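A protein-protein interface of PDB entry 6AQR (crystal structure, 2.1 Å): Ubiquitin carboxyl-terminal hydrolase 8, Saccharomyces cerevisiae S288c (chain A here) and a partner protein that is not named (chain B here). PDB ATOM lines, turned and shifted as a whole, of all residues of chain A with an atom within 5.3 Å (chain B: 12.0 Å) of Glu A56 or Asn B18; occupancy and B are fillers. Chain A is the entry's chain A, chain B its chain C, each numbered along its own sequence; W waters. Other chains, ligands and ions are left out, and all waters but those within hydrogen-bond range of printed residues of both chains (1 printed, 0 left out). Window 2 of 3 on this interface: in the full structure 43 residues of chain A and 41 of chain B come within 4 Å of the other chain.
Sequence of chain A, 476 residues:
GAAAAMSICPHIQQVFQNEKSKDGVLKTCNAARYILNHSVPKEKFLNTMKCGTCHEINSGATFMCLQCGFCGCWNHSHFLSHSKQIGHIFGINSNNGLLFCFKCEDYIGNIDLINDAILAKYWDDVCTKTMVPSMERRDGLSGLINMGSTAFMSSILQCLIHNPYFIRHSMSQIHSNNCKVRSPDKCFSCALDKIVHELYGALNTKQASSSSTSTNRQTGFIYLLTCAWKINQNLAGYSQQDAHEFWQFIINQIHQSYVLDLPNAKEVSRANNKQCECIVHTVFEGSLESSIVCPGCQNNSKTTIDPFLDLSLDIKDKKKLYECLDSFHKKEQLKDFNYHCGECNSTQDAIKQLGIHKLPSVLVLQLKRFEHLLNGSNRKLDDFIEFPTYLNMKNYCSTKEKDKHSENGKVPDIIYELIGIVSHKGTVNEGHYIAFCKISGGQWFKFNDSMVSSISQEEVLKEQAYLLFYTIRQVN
Lys A50 touches none of the printed residues of chain B. No residue of chain B comes within 4 Å of Cys A54. No residue of chain B comes within 4 Å of His A55. Of chain B, only Asn B18 (3.0 Å) comes within 4 Å of Glu A56. Ile A57 touches just one residue of chain B: Asn B18 (3.1 Å). Of chain B, only Asn B18 (3.1 Å), Leu B19 (3.9 Å) and Thr B22 (3.1 Å) come within 4 Å of Asn A58. Ser A59 touches just one residue of chain B: Asn B18. Gly A60 touches just these residues of chain B: Thr B21, Thr B22 and Gln B25. Of the printed residues of chain B, Asn A75 touches Thr B21 (3.1 Å) and Gln B25 (3.1 Å). Ser B12 touches none of the printed residues of chain A. Gly B14 touches none of the printed residues of chain A. Printed residues of chain A within 4 Å of Leu B19: Asn A58. Of the printed residues of chain A, Thr B21 touches Gly A60 and Asn A75. Printed residues of chain A within 4 Å of Thr B22: Asn A58 (3.1 Å) and Gly A60 (3.0 Å). Printed residues of chain A within 4 Å of Gln B25: Gly A60 (3.6 Å) and Asn A75 (3.1 Å). The nearest printed residue of chain A that does not touch Thr B21 is Asn A58 (4.7 Å).
The side-chain carboxylate (OE1) of Glu A56 lies within hydrogen-bond range of the side-chain amide nitrogen (ND2) of Asn B18 (3.0 Å). The backbone carbonyl oxygen of Ile A57 is in hydrogen-bond range of the side-chain amide nitrogen of Asn B18. O of Asn A58 is in hydrogen-bond range of OG1 of Thr B22 (3.1 Å). O of Gly A60 sits at hydrogen-bond distance from OG1 of Thr B22, at 3.0 Å. The side-chain hydroxyl of Thr B21 sits at hydrogen-bond distance from the side-chain amide nitrogen of Asn A75 (3.1 Å). OD1 of Asn A75 sits at hydrogen-bond distance from NE2 of Gln B25. The backbone carbonyl oxygen (O) of Asn A58 sits close to the backbone carbonyl oxygen (O) of Asn B18 (3.1 Å).
Water W1 lies within hydrogen-bond range of OD1 of Asn B18 (2.9 Å), OG of Ser A59 (3.1 Å) and ND2 of Asn A75 (3.2 Å).
O of Met A49 is in hydrogen-bond range of N of Asn A58. The backbone NH (N) of Cys A51 is in hydrogen-bond range of the backbone carbonyl oxygen (O) of Glu A56 (3.1 Å). The backbone NH (N) of Gly A60 lies close to the side-chain amide nitrogen (ND2) of Asn A75. The backbone carbonyl oxygen of Asn B17 sits at hydrogen-bond distance from the side-chain hydroxyl of Thr B21. The side-chain hydroxyl of Thr B22 sits at hydrogen-bond distance from the backbone carbonyl oxygen of Asn B18 (2.8 Å). The backbone carbonyl oxygen of Thr B21 sits close to the side-chain amide nitrogen of Gln B25, 3.2 Å away.
Printed residues of chain A that touch a printed residue of chain B: Glu A56, Ile A57, Asn A58, Ser A59, Gly A60 and Asn A75. Among the printed residues, 11 pairs touch across the chains.
Among the printed residues, pairs that only touch across the chains: Asn A58 with Leu B19, Ser A59 with Asn B18, Gly A60 with Thr B21 and Gly A60 with Gln B25.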
ATOM      1  N   MET A  49      -8.633  -3.357  -5.074  1.00  0.00           N
ATOM      2  CA  MET A  49      -8.722  -3.867  -3.729  1.00  0.00           C
ATOM      3  C   MET A  49      -9.316  -2.902  -2.668  1.00  0.00           C
ATOM      4  O   MET A  49      -9.098  -3.072  -1.472  1.00  0.00           O
ATOM      5  CB  MET A  49      -7.361  -4.462  -3.300  1.00  0.00           C
ATOM      6  CG  MET A  49      -7.024  -5.731  -4.087  1.00  0.00           C
ATOM      7  SD  MET A  49      -5.274  -6.100  -3.990  1.00  0.00           S
ATOM      8  CE  MET A  49      -5.090  -7.309  -5.335  1.00  0.00           C
ATOM      9  N   LYS A  50     -10.110  -1.939  -3.118  1.00  0.00           N
ATOM     10  CA  LYS A  50     -10.629  -0.950  -2.232  1.00  0.00           C
ATOM     11  C   LYS A  50     -12.151  -1.038  -2.286  1.00  0.00           C
ATOM     12  O   LYS A  50     -12.718  -0.908  -3.337  1.00  0.00           O
ATOM     13  CB  LYS A  50     -10.132   0.430  -2.631  1.00  0.00           C
ATOM     14  CG  LYS A  50     -10.585   1.534  -1.704  1.00  0.00           C
ATOM     15  CD  LYS A  50     -10.325   2.873  -2.392  1.00  0.00           C
ATOM     16  CE  LYS A  50     -10.296   3.992  -1.388  1.00  0.00           C
ATOM     17  NZ  LYS A  50     -10.336   5.293  -2.138  1.00  0.00           N
ATOM     18  N   CYS A  51     -12.796  -1.278  -1.149  1.00  0.00           N
ATOM     19  CA  CYS A  51     -14.258  -1.501  -1.173  1.00  0.00           C
ATOM     20  C   CYS A  51     -14.942  -0.181  -1.500  1.00  0.00           C
ATOM     21  O   CYS A  51     -14.581   0.825  -0.919  1.00  0.00           O
ATOM     22  CB  CYS A  51     -14.725  -1.970   0.185  1.00  0.00           C
ATOM     23  SG  CYS A  51     -16.471  -2.478   0.360  1.00  0.00           S
ATOM     24  N   CYS A  54     -17.006   0.629   2.340  1.00  0.00           N
ATOM     25  CA  CYS A  54     -16.273   0.985   3.535  1.00  0.00           C
ATOM     26  C   CYS A  54     -14.939   1.671   3.257  1.00  0.00           C
ATOM     27  O   CYS A  54     -14.309   2.159   4.198  1.00  0.00           O
ATOM     28  CB  CYS A  54     -16.060  -0.223   4.475  1.00  0.00           C
ATOM     29  SG  CYS A  54     -15.075  -1.619   3.811  1.00  0.00           S
ATOM     30  N   HIS A  55     -14.488   1.659   1.991  1.00  0.00           N
ATOM     31  CA  HIS A  55     -13.202   2.310   1.574  1.00  0.00           C
ATOM     32  C   HIS A  55     -11.934   1.719   2.146  1.00  0.00           C
ATOM     33  O   HIS A  55     -10.893   2.312   2.047  1.00  0.00           O
ATOM     34  CB  HIS A  55     -13.211   3.816   1.857  1.00  0.00           C
ATOM     35  CG  HIS A  55     -14.451   4.484   1.374  1.00  0.00           C
ATOM     36  ND1 HIS A  55     -14.793   4.542   0.032  1.00  0.00           N
ATOM     37  CD2 HIS A  55     -15.467   5.082   2.049  1.00  0.00           C
ATOM     38  CE1 HIS A  55     -15.950   5.174  -0.104  1.00  0.00           C
ATOM     39  NE2 HIS A  55     -16.388   5.497   1.106  1.00  0.00           N
ATOM     40  N   GLU A  56     -12.012   0.570   2.772  1.00  0.00           N
ATOM     41  CA  GLU A  56     -10.777  -0.057   3.247  1.00  0.00           C
ATOM     42  C   GLU A  56     -10.107  -0.908   2.128  1.00  0.00           C
ATOM     43  O   GLU A  56     -10.752  -1.480   1.196  1.00  0.00           O
ATOM     44  CB  GLU A  56     -11.027  -0.961   4.455  1.00  0.00           C
ATOM     45  CG  GLU A  56     -11.679  -0.367   5.684  1.00  0.00           C
ATOM     46  CD  GLU A  56     -11.737  -1.420   6.767  1.00  0.00           C
ATOM     47  OE1 GLU A  56     -10.695  -2.099   6.899  1.00  0.00           O
ATOM     48  OE2 GLU A  56     -12.799  -1.619   7.436  1.00  0.00           O
ATOM     49  N   ILE A  57      -8.802  -0.993   2.241  1.00  0.00           N
ATOM     50  CA  ILE A  57      -8.013  -1.792   1.340  1.00  0.00           C
ATOM     51  C   ILE A  57      -7.862  -3.154   1.955  1.00  0.00           C
ATOM     52  O   ILE A  57      -7.579  -3.267   3.154  1.00  0.00           O
ATOM     53  CB  ILE A  57      -6.674  -1.083   1.060  1.00  0.00           C
ATOM     54  CG1 ILE A  57      -7.016   0.193   0.233  1.00  0.00           C
ATOM     55  CG2 ILE A  57      -5.734  -2.044   0.297  1.00  0.00           C
ATOM     56  CD1 ILE A  57      -6.032   1.281   0.432  1.00  0.00           C
ATOM     57  N   ASN A  58      -8.075  -4.198   1.136  1.00  0.00           N
ATOM     58  CA  ASN A  58      -7.912  -5.588   1.595  1.00  0.00           C
ATOM     59  C   ASN A  58      -8.737  -5.929   2.834  1.00  0.00           C
ATOM     60  O   ASN A  58      -8.245  -6.591   3.768  1.00  0.00           O
ATOM     61  CB  ASN A  58      -6.442  -5.903   1.876  1.00  0.00           C
ATOM     62  CG  ASN A  58      -5.585  -5.976   0.628  1.00  0.00           C
ATOM     63  OD1 ASN A  58      -6.046  -6.336  -0.471  1.00  0.00           O
ATOM     64  ND2 ASN A  58      -4.284  -5.706   0.819  1.00  0.00           N
ATOM     65  N   SER A  59     -10.002  -5.527   2.847  1.00  0.00           N
ATOM     66  CA  SER A  59     -10.941  -5.960   3.888  1.00  0.00           C
ATOM     67  C   SER A  59     -11.377  -7.364   3.574  1.00  0.00           C
ATOM     68  O   SER A  59     -12.543  -7.620   3.159  1.00  0.00           O
ATOM     69  CB  SER A  59     -12.156  -4.975   3.930  1.00  0.00           C
ATOM     70  OG  SER A  59     -13.041  -5.333   4.958  1.00  0.00           O
ATOM     71  N   GLY A  60     -10.419  -8.292   3.682  1.00  0.00           N
ATOM     72  CA  GLY A  60     -10.544  -9.626   3.013  1.00  0.00           C
ATOM     73  C   GLY A  60     -10.450  -9.504   1.467  1.00  0.00           C
ATOM     74  O   GLY A  60      -9.990  -8.511   0.943  1.00  0.00           O
ATOM     75  N   ASN A  75     -14.892  -9.027   4.141  1.00  0.00           N
ATOM     76  CA  ASN A  75     -14.894  -9.073   5.628  1.00  0.00           C
ATOM     77  C   ASN A  75     -16.108  -8.374   6.299  1.00  0.00           C
ATOM     78  O   ASN A  75     -16.544  -8.820   7.341  1.00  0.00           O
ATOM     79  CB  ASN A  75     -13.567  -8.572   6.225  1.00  0.00           C
ATOM     80  CG  ASN A  75     -12.447  -9.636   6.168  1.00  0.00           C
ATOM     81  OD1 ASN A  75     -12.578 -10.703   5.554  1.00  0.00           O
ATOM     82  ND2 ASN A  75     -11.334  -9.315   6.749  1.00  0.00           N
ATOM     83  N   HIS A  76     -16.637  -7.323   5.658  1.00  0.00           N
ATOM     84  CA  HIS A  76     -17.801  -6.608   6.120  1.00  0.00           C
ATOM     85  C   HIS A  76     -19.019  -6.884   5.286  1.00  0.00           C
ATOM     86  O   HIS A  76     -19.963  -6.147   5.360  1.00  0.00           O
ATOM     87  CB  HIS A  76     -17.540  -5.087   6.133  1.00  0.00           C
ATOM     88  CG  HIS A  76     -16.353  -4.679   6.950  1.00  0.00           C
ATOM     89  ND1 HIS A  76     -16.060  -5.245   8.173  1.00  0.00           N
ATOM     90  CD2 HIS A  76     -15.386  -3.752   6.725  1.00  0.00           C
ATOM     91  CE1 HIS A  76     -14.952  -4.705   8.662  1.00  0.00           C
ATOM     92  NE2 HIS A  76     -14.531  -3.784   7.812  1.00  0.00           N
ATOM     93  N   ASP B   9      -1.397   0.305  18.382  1.00  0.00           N
ATOM     94  CA  ASP B   9      -1.659  -1.150  18.361  1.00  0.00           C
ATOM     95  C   ASP B   9      -3.014  -1.585  17.802  1.00  0.00           C
ATOM     96  O   ASP B   9      -3.084  -2.584  17.107  1.00  0.00           O
ATOM     97  CB  ASP B   9      -1.513  -1.761  19.750  1.00  0.00           C
ATOM     98  CG  ASP B   9      -0.095  -1.911  20.160  1.00  0.00           C
ATOM     99  OD1 ASP B   9       0.781  -1.468  19.387  1.00  0.00           O
ATOM    100  OD2 ASP B   9       0.160  -2.461  21.265  1.00  0.00           O
ATOM    101  N   SER B  10      -4.078  -0.862  18.129  1.00  0.00           N
ATOM    102  CA  SER B  10      -5.398  -1.114  17.564  1.00  0.00           C
ATOM    103  C   SER B  10      -5.304  -1.148  16.028  1.00  0.00           C
ATOM    104  O   SER B  10      -5.561  -2.172  15.397  1.00  0.00           O
ATOM    105  CB  SER B  10      -6.376   0.002  18.017  1.00  0.00           C
ATOM    106  OG  SER B  10      -7.545   0.112  17.194  1.00  0.00           O
ATOM    107  N   ILE B  11      -4.952   0.002  15.456  1.00  0.00           N
ATOM    108  CA  ILE B  11      -4.880   0.174  14.043  1.00  0.00           C
ATOM    109  C   ILE B  11      -3.824  -0.766  13.400  1.00  0.00           C
ATOM    110  O   ILE B  11      -4.144  -1.438  12.429  1.00  0.00           O
ATOM    111  CB  ILE B  11      -4.812   1.658  13.664  1.00  0.00           C
ATOM    112  CG1 ILE B  11      -6.230   2.206  13.781  1.00  0.00           C
ATOM    113  CG2 ILE B  11      -4.352   1.808  12.229  1.00  0.00           C
ATOM    114  CD1 ILE B  11      -6.339   3.676  13.482  1.00  0.00           C
ATOM    115  N   SER B  12      -2.642  -0.887  13.996  1.00  0.00           N
ATOM    116  CA  SER B  12      -1.659  -1.825  13.493  1.00  0.00           C
ATOM    117  C   SER B  12      -2.229  -3.240  13.324  1.00  0.00           C
ATOM    118  O   SER B  12      -1.999  -3.855  12.287  1.00  0.00           O
ATOM    119  CB  SER B  12      -0.421  -1.841  14.353  1.00  0.00           C
ATOM    120  OG  SER B  12       0.228  -0.576  14.223  1.00  0.00           O
ATOM    121  N   ASN B  13      -3.003  -3.713  14.306  1.00  0.00           N
ATOM    122  CA  ASN B  13      -3.556  -5.066  14.297  1.00  0.00           C
ATOM    123  C   ASN B  13      -4.576  -5.171  13.241  1.00  0.00           C
ATOM    124  O   ASN B  13      -4.675  -6.200  12.621  1.00  0.00           O
ATOM    125  CB  ASN B  13      -4.256  -5.453  15.629  1.00  0.00           C
ATOM    126  CG  ASN B  13      -3.290  -5.737  16.742  1.00  0.00           C
ATOM    127  OD1 ASN B  13      -2.145  -6.174  16.531  1.00  0.00           O
ATOM    128  ND2 ASN B  13      -3.756  -5.503  17.971  1.00  0.00           N
ATOM    129  N   GLY B  14      -5.395  -4.145  13.101  1.00  0.00           N
ATOM    130  CA  GLY B  14      -6.435  -4.126  12.063  1.00  0.00           C
ATOM    131  C   GLY B  14      -5.803  -4.224  10.661  1.00  0.00           C
ATOM    132  O   GLY B  14      -6.354  -4.869   9.786  1.00  0.00           O
ATOM    133  N   ILE B  15      -4.629  -3.603  10.456  1.00  0.00           N
ATOM    134  CA  ILE B  15      -4.058  -3.509   9.141  1.00  0.00           C
ATOM    135  C   ILE B  15      -3.485  -4.893   8.862  1.00  0.00           C
ATOM    136  O   ILE B  15      -3.714  -5.455   7.789  1.00  0.00           O
ATOM    137  CB  ILE B  15      -2.978  -2.399   9.047  1.00  0.00           C
ATOM    138  CG1 ILE B  15      -3.644  -1.032   8.932  1.00  0.00           C
ATOM    139  CG2 ILE B  15      -2.001  -2.688   7.885  1.00  0.00           C
ATOM    140  CD1 ILE B  15      -2.704   0.076   9.230  1.00  0.00           C
ATOM    141  N   LEU B  16      -2.788  -5.459   9.836  1.00  0.00           N
ATOM    142  CA  LEU B  16      -2.276  -6.777   9.677  1.00  0.00           C
ATOM    143  C   LEU B  16      -3.403  -7.821   9.434  1.00  0.00           C
ATOM    144  O   LEU B  16      -3.219  -8.740   8.643  1.00  0.00           O
ATOM    145  CB  LEU B  16      -1.426  -7.163  10.861  1.00  0.00           C
ATOM    146  CG  LEU B  16      -0.945  -8.596  10.970  1.00  0.00           C
ATOM    147  CD1 LEU B  16       0.032  -8.952   9.850  1.00  0.00           C
ATOM    148  CD2 LEU B  16      -0.313  -8.859  12.329  1.00  0.00           C
ATOM    149  N   ASN B  17      -4.570  -7.650  10.065  1.00  0.00           N
ATOM    150  CA  ASN B  17      -5.590  -8.657   9.988  1.00  0.00           C
ATOM    151  C   ASN B  17      -6.231  -8.530   8.593  1.00  0.00           C
ATOM    152  O   ASN B  17      -6.646  -9.518   8.046  1.00  0.00           O
ATOM    153  CB  ASN B  17      -6.605  -8.481  11.134  1.00  0.00           C
ATOM    154  CG  ASN B  17      -7.794  -9.412  11.013  1.00  0.00           C
ATOM    155  OD1 ASN B  17      -8.893  -9.025  10.563  1.00  0.00           O
ATOM    156  ND2 ASN B  17      -7.577 -10.653  11.363  1.00  0.00           N
ATOM    157  N   ASN B  18      -6.307  -7.315   8.031  1.00  0.00           N
ATOM    158  CA  ASN B  18      -6.698  -7.139   6.631  1.00  0.00           C
ATOM    159  C   ASN B  18      -5.759  -7.917   5.647  1.00  0.00           C
ATOM    160  O   ASN B  18      -6.223  -8.645   4.783  1.00  0.00           O
ATOM    161  CB  ASN B  18      -6.780  -5.634   6.289  1.00  0.00           C
ATOM    162  CG  ASN B  18      -8.131  -5.018   6.682  1.00  0.00           C
ATOM    163  OD1 ASN B  18      -8.834  -5.528   7.507  1.00  0.00           O
ATOM    164  ND2 ASN B  18      -8.493  -3.942   6.054  1.00  0.00           N
ATOM    165  N   LEU B  19      -4.444  -7.762   5.811  1.00  0.00           N
ATOM    166  CA  LEU B  19      -3.461  -8.468   4.998  1.00  0.00           C
ATOM    167  C   LEU B  19      -3.541  -9.977   5.164  1.00  0.00           C
ATOM    168  O   LEU B  19      -3.517 -10.715   4.162  1.00  0.00           O
ATOM    169  CB  LEU B  19      -2.037  -7.999   5.360  1.00  0.00           C
ATOM    170  CG  LEU B  19      -1.836  -6.545   4.987  1.00  0.00           C
ATOM    171  CD1 LEU B  19      -0.646  -6.075   5.872  1.00  0.00           C
ATOM    172  CD2 LEU B  19      -1.592  -6.424   3.496  1.00  0.00           C
ATOM    173  N   LEU B  20      -3.661 -10.438   6.406  1.00  0.00           N
ATOM    174  CA  LEU B  20      -3.669 -11.894   6.700  1.00  0.00           C
ATOM    175  C   LEU B  20      -4.904 -12.586   6.158  1.00  0.00           C
ATOM    176  O   LEU B  20      -4.793 -13.638   5.524  1.00  0.00           O
ATOM    177  CB  LEU B  20      -3.511 -12.197   8.184  1.00  0.00           C
ATOM    178  CG  LEU B  20      -2.070 -12.046   8.682  1.00  0.00           C
ATOM    179  CD1 LEU B  20      -2.063 -12.183  10.230  1.00  0.00           C
ATOM    180  CD2 LEU B  20      -1.110 -13.059   8.011  1.00  0.00           C
ATOM    181  N   THR B  21      -6.063 -11.979   6.373  1.00  0.00           N
ATOM    182  CA  THR B  21      -7.322 -12.611   5.941  1.00  0.00           C
ATOM    183  C   THR B  21      -7.449 -12.569   4.405  1.00  0.00           C
ATOM    184  O   THR B  21      -8.040 -13.453   3.824  1.00  0.00           O
ATOM    185  CB  THR B  21      -8.577 -11.921   6.593  1.00  0.00           C
ATOM    186  OG1 THR B  21      -8.533 -10.483   6.359  1.00  0.00           O
ATOM    187  CG2 THR B  21      -8.627 -12.242   8.078  1.00  0.00           C
ATOM    188  N   THR B  22      -6.939 -11.496   3.767  1.00  0.00           N
ATOM    189  CA  THR B  22      -6.866 -11.415   2.343  1.00  0.00           C
ATOM    190  C   THR B  22      -6.054 -12.528   1.758  1.00  0.00           C
ATOM    191  O   THR B  22      -6.500 -13.203   0.798  1.00  0.00           O
ATOM    192  CB  THR B  22      -6.368 -10.027   1.827  1.00  0.00           C
ATOM    193  OG1 THR B  22      -7.350  -9.070   2.205  1.00  0.00           O
ATOM    194  CG2 THR B  22      -6.273 -10.007   0.238  1.00  0.00           C
ATOM    195  N   LEU B  23      -4.873 -12.736   2.319  1.00  0.00           N
ATOM    196  CA  LEU B  23      -4.009 -13.755   1.859  1.00  0.00           C
ATOM    197  C   LEU B  23      -4.613 -15.140   2.135  1.00  0.00           C
ATOM    198  O   LEU B  23      -4.546 -16.022   1.250  1.00  0.00           O
ATOM    199  CB  LEU B  23      -2.666 -13.661   2.554  1.00  0.00           C
ATOM    200  CG  LEU B  23      -1.681 -14.768   2.184  1.00  0.00           C
ATOM    201  CD1 LEU B  23      -1.366 -14.806   0.685  1.00  0.00           C
ATOM    202  CD2 LEU B  23      -0.343 -14.580   2.942  1.00  0.00           C
ATOM    203  N   ILE B  24      -5.182 -15.348   3.316  1.00  0.00           N
ATOM    204  CA  ILE B  24      -5.828 -16.678   3.611  1.00  0.00           C
ATOM    205  C   ILE B  24      -6.928 -16.981   2.570  1.00  0.00           C
ATOM    206  O   ILE B  24      -6.975 -18.042   2.016  1.00  0.00           O
ATOM    207  CB  ILE B  24      -6.404 -16.756   5.053  1.00  0.00           C
ATOM    208  CG1 ILE B  24      -5.236 -16.756   6.029  1.00  0.00           C
ATOM    209  CG2 ILE B  24      -7.227 -18.055   5.280  1.00  0.00           C
ATOM    210  CD1 ILE B  24      -5.591 -16.510   7.460  1.00  0.00           C
ATOM    211  N   GLN B  25      -7.825 -16.022   2.362  1.00  0.00           N
ATOM    212  CA  GLN B  25      -8.936 -16.144   1.419  1.00  0.00           C
ATOM    213  C   GLN B  25      -8.518 -16.403  -0.030  1.00  0.00           C
ATOM    214  O   GLN B  25      -9.222 -17.100  -0.782  1.00  0.00           O
ATOM    215  CB  GLN B  25      -9.804 -14.890   1.515  1.00  0.00           C
ATOM    216  CG  GLN B  25     -10.569 -14.922   2.821  1.00  0.00           C
ATOM    217  CD  GLN B  25     -11.195 -13.575   3.156  1.00  0.00           C
ATOM    218  OE1 GLN B  25     -11.698 -12.910   2.289  1.00  0.00           O
ATOM    219  NE2 GLN B  25     -11.131 -13.161   4.416  1.00  0.00           N
ATOM    220  N   ASP B  26      -7.369 -15.832  -0.421  1.00  0.00           N
ATOM    221  CA  ASP B  26      -6.771 -16.097  -1.729  1.00  0.00           C
ATOM    222  C   ASP B  26      -6.288 -17.577  -1.815  1.00  0.00           C
ATOM    223  O   ASP B  26      -6.653 -18.335  -2.737  1.00  0.00           O
ATOM    224  CB  ASP B  26      -5.598 -15.110  -1.972  1.00  0.00           C
ATOM    225  CG  ASP B  26      -4.876 -15.350  -3.336  1.00  0.00           C
ATOM    226  OD1 ASP B  26      -3.744 -14.821  -3.467  1.00  0.00           O
ATOM    227  OD2 ASP B  26      -5.417 -16.004  -4.294  1.00  0.00           O
ATOM    228  N   ILE B  27      -5.443 -17.982  -0.873  1.00  0.00           N
ATOM    229  CA  ILE B  27      -4.975 -19.376  -0.882  1.00  0.00           C
ATOM    230  C   ILE B  27      -6.161 -20.378  -0.856  1.00  0.00           C
ATOM    231  O   ILE B  27      -6.214 -21.315  -1.685  1.00  0.00           O
ATOM    232  CB  ILE B  27      -4.088 -19.648   0.313  1.00  0.00           C
ATOM    233  CG1 ILE B  27      -2.771 -18.852   0.221  1.00  0.00           C
ATOM    234  CG2 ILE B  27      -3.839 -21.193   0.428  1.00  0.00           C
ATOM    235  CD1 ILE B  27      -2.101 -18.739   1.622  1.00  0.00           C
HETATM  236  O   HOH W   1     -11.669  -6.283   7.579  1.00  0.00           O
